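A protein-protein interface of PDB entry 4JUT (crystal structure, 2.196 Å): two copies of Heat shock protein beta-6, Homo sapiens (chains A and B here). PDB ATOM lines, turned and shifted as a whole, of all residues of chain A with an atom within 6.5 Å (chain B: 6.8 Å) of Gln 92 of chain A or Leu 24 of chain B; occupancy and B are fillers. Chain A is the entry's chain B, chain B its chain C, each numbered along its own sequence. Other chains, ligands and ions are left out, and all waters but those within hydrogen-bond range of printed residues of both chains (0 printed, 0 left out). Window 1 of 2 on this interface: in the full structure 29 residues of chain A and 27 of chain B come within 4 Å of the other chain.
Of the printed residues of chain B, Ser 81 of chain A touches Val 11 (3.7 Å). Ile 91 of chain A touches none of the printed residues of chain B. Of the printed residues of chain B, Gln 92 of chain A touches Leu 24 (3.8 Å). Of chain A, only Ser 90 (3.5 Å) and Gln 92 (3.8 Å) come within 4 Å of Leu 24 of chain B. Printed residues of chain A within 4 Å of Asp 26 of chain B: Leu 24 (3.6 Å). The nearest residue of chain B that does not touch Gln 92 of chain A is Gln 92 of chain B (5.5 Å). The nearest residue of chain A that does not touch Leu 24 of chain B is Leu 24 of chain A (4.1 Å). The nearest printed residue of chain B that does not touch Val 23 of chain A is Leu 24 of chain B (6.3 Å).
NE2 of Gln 92 of chain A sits at hydrogen-bond distance from NE2 of His 20 of chain A, at 2.9 Å. The backbone carbonyl oxygen of Ile 91 of chain A lies within hydrogen-bond range of the backbone NH of Val 23 of chain A, at 2.9 Å. O of Gln 92 of chain A is in hydrogen-bond range of N of Thr 80 of chain A (3.0 Å). OG of Ser 90 of chain A sits at hydrogen-bond distance from OE1 of Gln 92 of chain A. The backbone NH (N) of Leu 89 of chain B lies within hydrogen-bond range of the backbone carbonyl oxygen (O) of Leu 25 of chain B (2.8 Å).
Ser 90 of chain A touches Leu 24 of chain B, but with the chains exchanged Leu 24 of chain A does not touch Ser 90 of chain B (7.7 Å). Gln 92 of chain A touches Leu 24 of chain B, but with the chains exchanged Leu 24 of chain A does not touch Gln 92 of chain B (11.1 Å). Of the 10 pairs that touch across the chains among the printed residues, none has its exchanged pair printed and touching as well.
Among the printed residues, merely in contact across the chains: Ser 22 of chain A with Val 88 of chain B (3.2 Å), Val 79 of chain A with Val 11 of chain B (3.4 Å), Ser 90 of chain A with Leu 24 of chain B (3.5 Å), Thr 80 of chain A with Val 11 of chain B (3.6 Å), Leu 24 of chain A with Asp 26 of chain B (3.6 Å), Leu 24 of chain A with Leu 25 of chain B (3.7 Å), Ser 81 of chain A with Val 11 of chain B (3.7 Å), Leu 24 of chain A with Val 88 of chain B (3.7 Å), Val 23 of chain A with Val 88 of chain B (3.7 Å) and Gln 92 of chain A with Leu 24 of chain B (3.8 Å).
Of the 13 printed residues of chain B, 5 touch a printed residue of chain A. Hydrophobic or aromatic side chains of chain B that line the printed part of chain A: Val 11, Leu 24 and Val 88. Printed residues of chain A that touch a printed residue of chain B: Ser 22, Val 23, Leu 24, Val 79, Thr 80, Ser 81, Ser 90 and Gln 92. Among the printed residues, 10 pairs touch across the chains.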
ATOM      1  N   HIS A  20      -7.667  -6.976 -14.723  1.00  0.00           N
ATOM      2  CA  HIS A  20      -7.659  -7.688 -13.449  1.00  0.00           C
ATOM      3  C   HIS A  20      -6.566  -7.109 -12.531  1.00  0.00           C
ATOM      4  O   HIS A  20      -5.704  -6.382 -12.997  1.00  0.00           O
ATOM      5  CB  HIS A  20      -7.353  -9.170 -13.719  1.00  0.00           C
ATOM      6  CG  HIS A  20      -6.080  -9.386 -14.487  1.00  0.00           C
ATOM      7  ND1 HIS A  20      -6.060  -9.759 -15.817  1.00  0.00           N
ATOM      8  CD2 HIS A  20      -4.780  -9.255 -14.116  1.00  0.00           C
ATOM      9  CE1 HIS A  20      -4.805  -9.854 -16.227  1.00  0.00           C
ATOM     10  NE2 HIS A  20      -4.009  -9.553 -15.215  1.00  0.00           N
ATOM     11  N   PHE A  21      -6.594  -7.482 -11.252  1.00  0.00           N
ATOM     12  CA  PHE A  21      -5.497  -7.228 -10.302  1.00  0.00           C
ATOM     13  C   PHE A  21      -4.117  -7.477 -10.914  1.00  0.00           C
ATOM     14  O   PHE A  21      -3.841  -8.561 -11.418  1.00  0.00           O
ATOM     15  CB  PHE A  21      -5.660  -8.118  -9.062  1.00  0.00           C
ATOM     16  CG  PHE A  21      -4.623  -7.888  -8.002  1.00  0.00           C
ATOM     17  CD1 PHE A  21      -4.832  -6.941  -7.003  1.00  0.00           C
ATOM     18  CD2 PHE A  21      -3.446  -8.618  -7.998  1.00  0.00           C
ATOM     19  CE1 PHE A  21      -3.865  -6.710  -6.024  1.00  0.00           C
ATOM     20  CE2 PHE A  21      -2.476  -8.418  -7.015  1.00  0.00           C
ATOM     21  CZ  PHE A  21      -2.690  -7.457  -6.020  1.00  0.00           C
ATOM     22  N   SER A  22      -3.254  -6.465 -10.853  1.00  0.00           N
ATOM     23  CA  SER A  22      -1.899  -6.566 -11.365  1.00  0.00           C
ATOM     24  C   SER A  22      -1.036  -5.465 -10.746  1.00  0.00           C
ATOM     25  O   SER A  22      -1.386  -4.300 -10.831  1.00  0.00           O
ATOM     26  CB  SER A  22      -1.911  -6.426 -12.888  1.00  0.00           C
ATOM     27  OG  SER A  22      -0.608  -6.465 -13.419  1.00  0.00           O
ATOM     28  N   VAL A  23       0.076  -5.832 -10.111  1.00  0.00           N
ATOM     29  CA  VAL A  23       0.955  -4.835  -9.507  1.00  0.00           C
ATOM     30  C   VAL A  23       2.397  -5.040  -9.938  1.00  0.00           C
ATOM     31  O   VAL A  23       2.803  -6.159 -10.283  1.00  0.00           O
ATOM     32  CB  VAL A  23       0.853  -4.773  -7.935  1.00  0.00           C
ATOM     33  CG1 VAL A  23      -0.588  -4.658  -7.489  1.00  0.00           C
ATOM     34  CG2 VAL A  23       1.492  -5.980  -7.270  1.00  0.00           C
ATOM     35  N   LEU A  24       3.155  -3.949  -9.943  1.00  0.00           N
ATOM     36  CA  LEU A  24       4.586  -4.010 -10.189  1.00  0.00           C
ATOM     37  C   LEU A  24       5.323  -3.440  -8.982  1.00  0.00           C
ATOM     38  O   LEU A  24       5.001  -2.357  -8.503  1.00  0.00           O
ATOM     39  CB  LEU A  24       4.949  -3.234 -11.445  1.00  0.00           C
ATOM     40  CG  LEU A  24       4.349  -3.721 -12.776  1.00  0.00           C
ATOM     41  CD1 LEU A  24       4.549  -2.662 -13.907  1.00  0.00           C
ATOM     42  CD2 LEU A  24       4.963  -5.047 -13.177  1.00  0.00           C
ATOM     43  N   VAL A  44      -2.740 -10.465  -0.813  1.00  0.00           N
ATOM     44  CA  VAL A  44      -1.444 -10.968  -1.236  1.00  0.00           C
ATOM     45  C   VAL A  44      -0.407 -10.250  -0.401  1.00  0.00           C
ATOM     46  O   VAL A  44      -0.405  -9.038  -0.409  1.00  0.00           O
ATOM     47  CB  VAL A  44      -1.110 -10.575  -2.672  1.00  0.00           C
ATOM     48  CG1 VAL A  44       0.339 -10.920  -2.968  1.00  0.00           C
ATOM     49  CG2 VAL A  44      -2.016 -11.270  -3.648  1.00  0.00           C
ATOM     50  N   LEU A  70      -6.866  -8.284  -2.347  1.00  0.00           N
ATOM     51  CA  LEU A  70      -7.253  -8.957  -3.586  1.00  0.00           C
ATOM     52  C   LEU A  70      -8.690  -8.564  -3.906  1.00  0.00           C
ATOM     53  O   LEU A  70      -9.395  -8.063  -3.025  1.00  0.00           O
ATOM     54  CB  LEU A  70      -7.159 -10.482  -3.433  1.00  0.00           C
ATOM     55  CG  LEU A  70      -5.802 -11.176  -3.598  1.00  0.00           C
ATOM     56  CD1 LEU A  70      -5.937 -12.702  -3.331  1.00  0.00           C
ATOM     57  CD2 LEU A  70      -5.230 -10.911  -4.999  1.00  0.00           C
ATOM     58  N   ALA A  78      -4.811 -19.055  -8.330  1.00  0.00           N
ATOM     59  CA  ALA A  78      -4.755 -18.306  -9.578  1.00  0.00           C
ATOM     60  C   ALA A  78      -3.829 -17.085  -9.504  1.00  0.00           C
ATOM     61  O   ALA A  78      -3.403 -16.583 -10.537  1.00  0.00           O
ATOM     62  CB  ALA A  78      -6.157 -17.884 -10.010  1.00  0.00           C
ATOM     63  N   VAL A  79      -3.535 -16.592  -8.303  1.00  0.00           N
ATOM     64  CA  VAL A  79      -2.546 -15.512  -8.159  1.00  0.00           C
ATOM     65  C   VAL A  79      -1.166 -16.009  -8.597  1.00  0.00           C
ATOM     66  O   VAL A  79      -0.706 -17.052  -8.137  1.00  0.00           O
ATOM     67  CB  VAL A  79      -2.474 -14.978  -6.707  1.00  0.00           C
ATOM     68  CG1 VAL A  79      -1.409 -13.844  -6.546  1.00  0.00           C
ATOM     69  CG2 VAL A  79      -3.843 -14.509  -6.250  1.00  0.00           C
ATOM     70  N   THR A  80      -0.520 -15.270  -9.498  1.00  0.00           N
ATOM     71  CA  THR A  80       0.810 -15.629 -10.005  1.00  0.00           C
ATOM     72  C   THR A  80       1.806 -14.488  -9.813  1.00  0.00           C
ATOM     73  O   THR A  80       1.419 -13.339  -9.587  1.00  0.00           O
ATOM     74  CB  THR A  80       0.795 -15.992 -11.521  1.00  0.00           C
ATOM     75  OG1 THR A  80       0.474 -14.834 -12.297  1.00  0.00           O
ATOM     76  CG2 THR A  80      -0.220 -17.085 -11.815  1.00  0.00           C
ATOM     77  N   SER A  81       3.088 -14.807  -9.922  1.00  0.00           N
ATOM     78  CA  SER A  81       4.128 -13.800  -9.793  1.00  0.00           C
ATOM     79  C   SER A  81       5.327 -14.128 -10.662  1.00  0.00           C
ATOM     80  O   SER A  81       5.637 -15.287 -10.898  1.00  0.00           O
ATOM     81  CB  SER A  81       4.549 -13.626  -8.325  1.00  0.00           C
ATOM     82  OG  SER A  81       5.664 -14.429  -7.992  1.00  0.00           O
ATOM     83  N   SER A  90       6.257  -8.770 -10.754  1.00  0.00           N
ATOM     84  CA  SER A  90       4.899  -8.656 -11.238  1.00  0.00           C
ATOM     85  C   SER A  90       3.999  -9.655 -10.514  1.00  0.00           C
ATOM     86  O   SER A  90       4.311 -10.832 -10.451  1.00  0.00           O
ATOM     87  CB  SER A  90       4.845  -8.901 -12.746  1.00  0.00           C
ATOM     88  OG  SER A  90       3.498  -9.146 -13.130  1.00  0.00           O
ATOM     89  N   ILE A  91       2.888  -9.181  -9.962  1.00  0.00           N
ATOM     90  CA  ILE A  91       1.910 -10.057  -9.325  1.00  0.00           C
ATOM     91  C   ILE A  91       0.535  -9.824  -9.941  1.00  0.00           C
ATOM     92  O   ILE A  91       0.060  -8.692 -10.018  1.00  0.00           O
ATOM     93  CB  ILE A  91       1.826  -9.814  -7.795  1.00  0.00           C
ATOM     94  CG1 ILE A  91       3.195  -9.975  -7.141  1.00  0.00           C
ATOM     95  CG2 ILE A  91       0.829 -10.765  -7.142  1.00  0.00           C
ATOM     96  CD1 ILE A  91       3.212  -9.561  -5.693  1.00  0.00           C
ATOM     97  N   GLN A  92      -0.105 -10.895 -10.388  1.00  0.00           N
ATOM     98  CA  GLN A  92      -1.363 -10.770 -11.098  1.00  0.00           C
ATOM     99  C   GLN A  92      -2.376 -11.758 -10.549  1.00  0.00           C
ATOM    100  O   GLN A  92      -1.986 -12.728  -9.910  1.00  0.00           O
ATOM    101  CB  GLN A  92      -1.136 -11.012 -12.587  1.00  0.00           C
ATOM    102  CG  GLN A  92      -0.162 -10.029 -13.193  1.00  0.00           C
ATOM    103  CD  GLN A  92      -0.064 -10.157 -14.696  1.00  0.00           C
ATOM    104  OE1 GLN A  92       1.031 -10.197 -15.251  1.00  0.00           O
ATOM    105  NE2 GLN A  92      -1.204 -10.199 -15.362  1.00  0.00           N
ATOM    106  N   ALA A  93      -3.663 -11.491 -10.787  1.00  0.00           N
ATOM    107  CA  ALA A  93      -4.755 -12.391 -10.392  1.00  0.00           C
ATOM    108  C   ALA A  93      -6.013 -12.117 -11.217  1.00  0.00           C
ATOM    109  O   ALA A  93      -6.108 -12.551 -12.366  1.00  0.00           O
ATOM    110  CB  ALA A  93      -5.063 -12.251  -8.906  1.00  0.00           C
ATOM    111  N   VAL B  11       2.874 -18.080  -3.537  1.00  0.00           N
ATOM    112  CA  VAL B  11       2.380 -17.757  -4.870  1.00  0.00           C
ATOM    113  C   VAL B  11       3.227 -18.421  -5.959  1.00  0.00           C
ATOM    114  O   VAL B  11       4.466 -18.384  -5.905  1.00  0.00           O
ATOM    115  CB  VAL B  11       2.282 -16.230  -5.090  1.00  0.00           C
ATOM    116  CG1 VAL B  11       2.066 -15.909  -6.558  1.00  0.00           C
ATOM    117  CG2 VAL B  11       1.159 -15.656  -4.248  1.00  0.00           C
ATOM    118  N   THR B  16       8.713 -14.773 -16.835  1.00  0.00           N
ATOM    119  CA  THR B  16       8.451 -13.417 -17.296  1.00  0.00           C
ATOM    120  C   THR B  16       7.967 -13.421 -18.756  1.00  0.00           C
ATOM    121  O   THR B  16       7.240 -12.518 -19.173  1.00  0.00           O
ATOM    122  CB  THR B  16       9.689 -12.500 -17.115  1.00  0.00           C
ATOM    123  OG1 THR B  16      10.200 -12.646 -15.784  1.00  0.00           O
ATOM    124  CG2 THR B  16       9.331 -11.033 -17.351  1.00  0.00           C
ATOM    125  N   SER B  22       3.914  -9.276 -24.802  1.00  0.00           N
ATOM    126  CA  SER B  22       3.395  -8.862 -23.507  1.00  0.00           C
ATOM    127  C   SER B  22       4.202  -7.704 -22.909  1.00  0.00           C
ATOM    128  O   SER B  22       5.428  -7.750 -22.848  1.00  0.00           O
ATOM    129  CB  SER B  22       3.371 -10.057 -22.554  1.00  0.00           C
ATOM    130  OG  SER B  22       2.338  -9.915 -21.598  1.00  0.00           O
ATOM    131  N   VAL B  23       3.510  -6.652 -22.489  1.00  0.00           N
ATOM    132  CA  VAL B  23       4.185  -5.486 -21.922  1.00  0.00           C
ATOM    133  C   VAL B  23       3.470  -5.040 -20.641  1.00  0.00           C
ATOM    134  O   VAL B  23       2.245  -5.009 -20.594  1.00  0.00           O
ATOM    135  CB  VAL B  23       4.283  -4.335 -22.964  1.00  0.00           C
ATOM    136  CG1 VAL B  23       4.609  -2.986 -22.295  1.00  0.00           C
ATOM    137  CG2 VAL B  23       5.333  -4.676 -24.023  1.00  0.00           C
ATOM    138  N   LEU B  24       4.237  -4.747 -19.593  1.00  0.00           N
ATOM    139  CA  LEU B  24       3.672  -4.229 -18.350  1.00  0.00           C
ATOM    140  C   LEU B  24       4.387  -2.931 -17.999  1.00  0.00           C
ATOM    141  O   LEU B  24       5.612  -2.843 -18.012  1.00  0.00           O
ATOM    142  CB  LEU B  24       3.785  -5.250 -17.194  1.00  0.00           C
ATOM    143  CG  LEU B  24       3.120  -6.626 -17.383  1.00  0.00           C
ATOM    144  CD1 LEU B  24       3.563  -7.652 -16.338  1.00  0.00           C
ATOM    145  CD2 LEU B  24       1.626  -6.489 -17.333  1.00  0.00           C
ATOM    146  N   LEU B  25       3.610  -1.909 -17.693  1.00  0.00           N
ATOM    147  CA  LEU B  25       4.181  -0.605 -17.396  1.00  0.00           C
ATOM    148  C   LEU B  25       3.445  -0.010 -16.212  1.00  0.00           C
ATOM    149  O   LEU B  25       2.209  -0.096 -16.127  1.00  0.00           O
ATOM    150  CB  LEU B  25       4.017   0.333 -18.595  1.00  0.00           C
ATOM    151  CG  LEU B  25       4.739  -0.001 -19.886  1.00  0.00           C
ATOM    152  CD1 LEU B  25       4.209   0.885 -21.019  1.00  0.00           C
ATOM    153  CD2 LEU B  25       6.238   0.203 -19.680  1.00  0.00           C
ATOM    154  N   ASP B  26       4.197   0.629 -15.324  1.00  0.00           N
ATOM    155  CA  ASP B  26       3.592   1.327 -14.199  1.00  0.00           C
ATOM    156  C   ASP B  26       3.135   2.739 -14.620  1.00  0.00           C
ATOM    157  O   ASP B  26       3.956   3.614 -14.904  1.00  0.00           O
ATOM    158  CB  ASP B  26       4.601   1.420 -13.049  1.00  0.00           C
ATOM    159  CG  ASP B  26       3.966   1.883 -11.747  1.00  0.00           C
ATOM    160  OD1 ASP B  26       2.895   2.523 -11.790  1.00  0.00           O
ATOM    161  OD2 ASP B  26       4.541   1.598 -10.675  1.00  0.00           O
ATOM    162  N   TYR B  68       7.402  -0.292 -29.068  1.00  0.00           N
ATOM    163  CA  TYR B  68       7.787  -1.697 -29.162  1.00  0.00           C
ATOM    164  C   TYR B  68       7.458  -2.263 -30.554  1.00  0.00           C
ATOM    165  O   TYR B  68       6.344  -2.096 -31.051  1.00  0.00           O
ATOM    166  CB  TYR B  68       7.039  -2.529 -28.125  1.00  0.00           C
ATOM    167  CG  TYR B  68       7.081  -1.997 -26.707  1.00  0.00           C
ATOM    168  CD1 TYR B  68       7.980  -2.504 -25.768  1.00  0.00           C
ATOM    169  CD2 TYR B  68       6.195  -1.010 -26.297  1.00  0.00           C
ATOM    170  CE1 TYR B  68       7.992  -2.022 -24.479  1.00  0.00           C
ATOM    171  CE2 TYR B  68       6.209  -0.523 -25.030  1.00  0.00           C
ATOM    172  CZ  TYR B  68       7.097  -1.027 -24.121  1.00  0.00           C
ATOM    173  OH  TYR B  68       7.062  -0.526 -22.852  1.00  0.00           O
ATOM    174  N   VAL B  88      -1.344  -0.560 -13.259  1.00  0.00           N
ATOM    175  CA  VAL B  88      -0.462  -1.251 -14.208  1.00  0.00           C
ATOM    176  C   VAL B  88      -1.128  -1.372 -15.575  1.00  0.00           C
ATOM    177  O   VAL B  88      -2.250  -1.871 -15.682  1.00  0.00           O
ATOM    178  CB  VAL B  88      -0.023  -2.659 -13.705  1.00  0.00           C
ATOM    179  CG1 VAL B  88       0.797  -3.430 -14.791  1.00  0.00           C
ATOM    180  CG2 VAL B  88       0.769  -2.511 -12.430  1.00  0.00           C
ATOM    181  N   LEU B  89      -0.426  -0.865 -16.593  1.00  0.00           N
ATOM    182  CA  LEU B  89      -0.840  -0.923 -17.982  1.00  0.00           C
ATOM    183  C   LEU B  89      -0.227  -2.160 -18.608  1.00  0.00           C
ATOM    184  O   LEU B  89       0.985  -2.333 -18.617  1.00  0.00           O
ATOM    185  CB  LEU B  89      -0.331   0.286 -18.768  1.00  0.00           C
ATOM    186  CG  LEU B  89      -0.735   0.265 -20.245  1.00  0.00           C
ATOM    187  CD1 LEU B  89      -2.252   0.391 -20.372  1.00  0.00           C
ATOM    188  CD2 LEU B  89      -0.017   1.330 -21.063  1.00  0.00           C
ATOM    189  N   SER B  90      -1.081  -3.006 -19.136  1.00  0.00           N
ATOM    190  CA  SER B  90      -0.639  -4.209 -19.835  1.00  0.00           C
ATOM    191  C   SER B  90      -1.008  -4.096 -21.304  1.00  0.00           C
ATOM    192  O   SER B  90      -2.097  -3.624 -21.646  1.00  0.00           O
ATOM    193  CB  SER B  90      -1.289  -5.458 -19.236  1.00  0.00           C
ATOM    194  OG  SER B  90      -2.687  -5.291 -19.239  1.00  0.00           O
ATOM    195  N   ILE B  91      -0.087  -4.501 -22.171  1.00  0.00           N
ATOM    196  CA  ILE B  91      -0.360  -4.539 -23.602  1.00  0.00           C
ATOM    197  C   ILE B  91      -0.010  -5.906 -24.171  1.00  0.00           C
ATOM    198  O   ILE B  91       1.109  -6.397 -24.002  1.00  0.00           O
ATOM    199  CB  ILE B  91       0.418  -3.470 -24.372  1.00  0.00           C
ATOM    200  CG1 ILE B  91       0.382  -2.139 -23.628  1.00  0.00           C
ATOM    201  CG2 ILE B  91      -0.181  -3.286 -25.752  1.00  0.00           C
ATOM    202  CD1 ILE B  91       1.204  -1.094 -24.288  1.00  0.00           C
ATOM    203  N   GLN B  92      -0.976  -6.508 -24.850  1.00  0.00           N
ATOM    204  CA  GLN B  92      -0.833  -7.867 -25.341  1.00  0.00           C
ATOM    205  C   GLN B  92      -1.366  -8.062 -26.754  1.00  0.00           C
ATOM    206  O   GLN B  92      -2.244  -7.334 -27.216  1.00  0.00           O
ATOM    207  CB  GLN B  92      -1.574  -8.815 -24.405  1.00  0.00           C
ATOM    208  CG  GLN B  92      -0.992  -8.865 -23.021  1.00  0.00           C
ATOM    209  CD  GLN B  92      -1.842  -9.674 -22.083  1.00  0.00           C
ATOM    210  OE1 GLN B  92      -2.929 -10.116 -22.453  1.00  0.00           O
ATOM    211  NE2 GLN B  92      -1.358  -9.881 -20.860  1.00  0.00           N
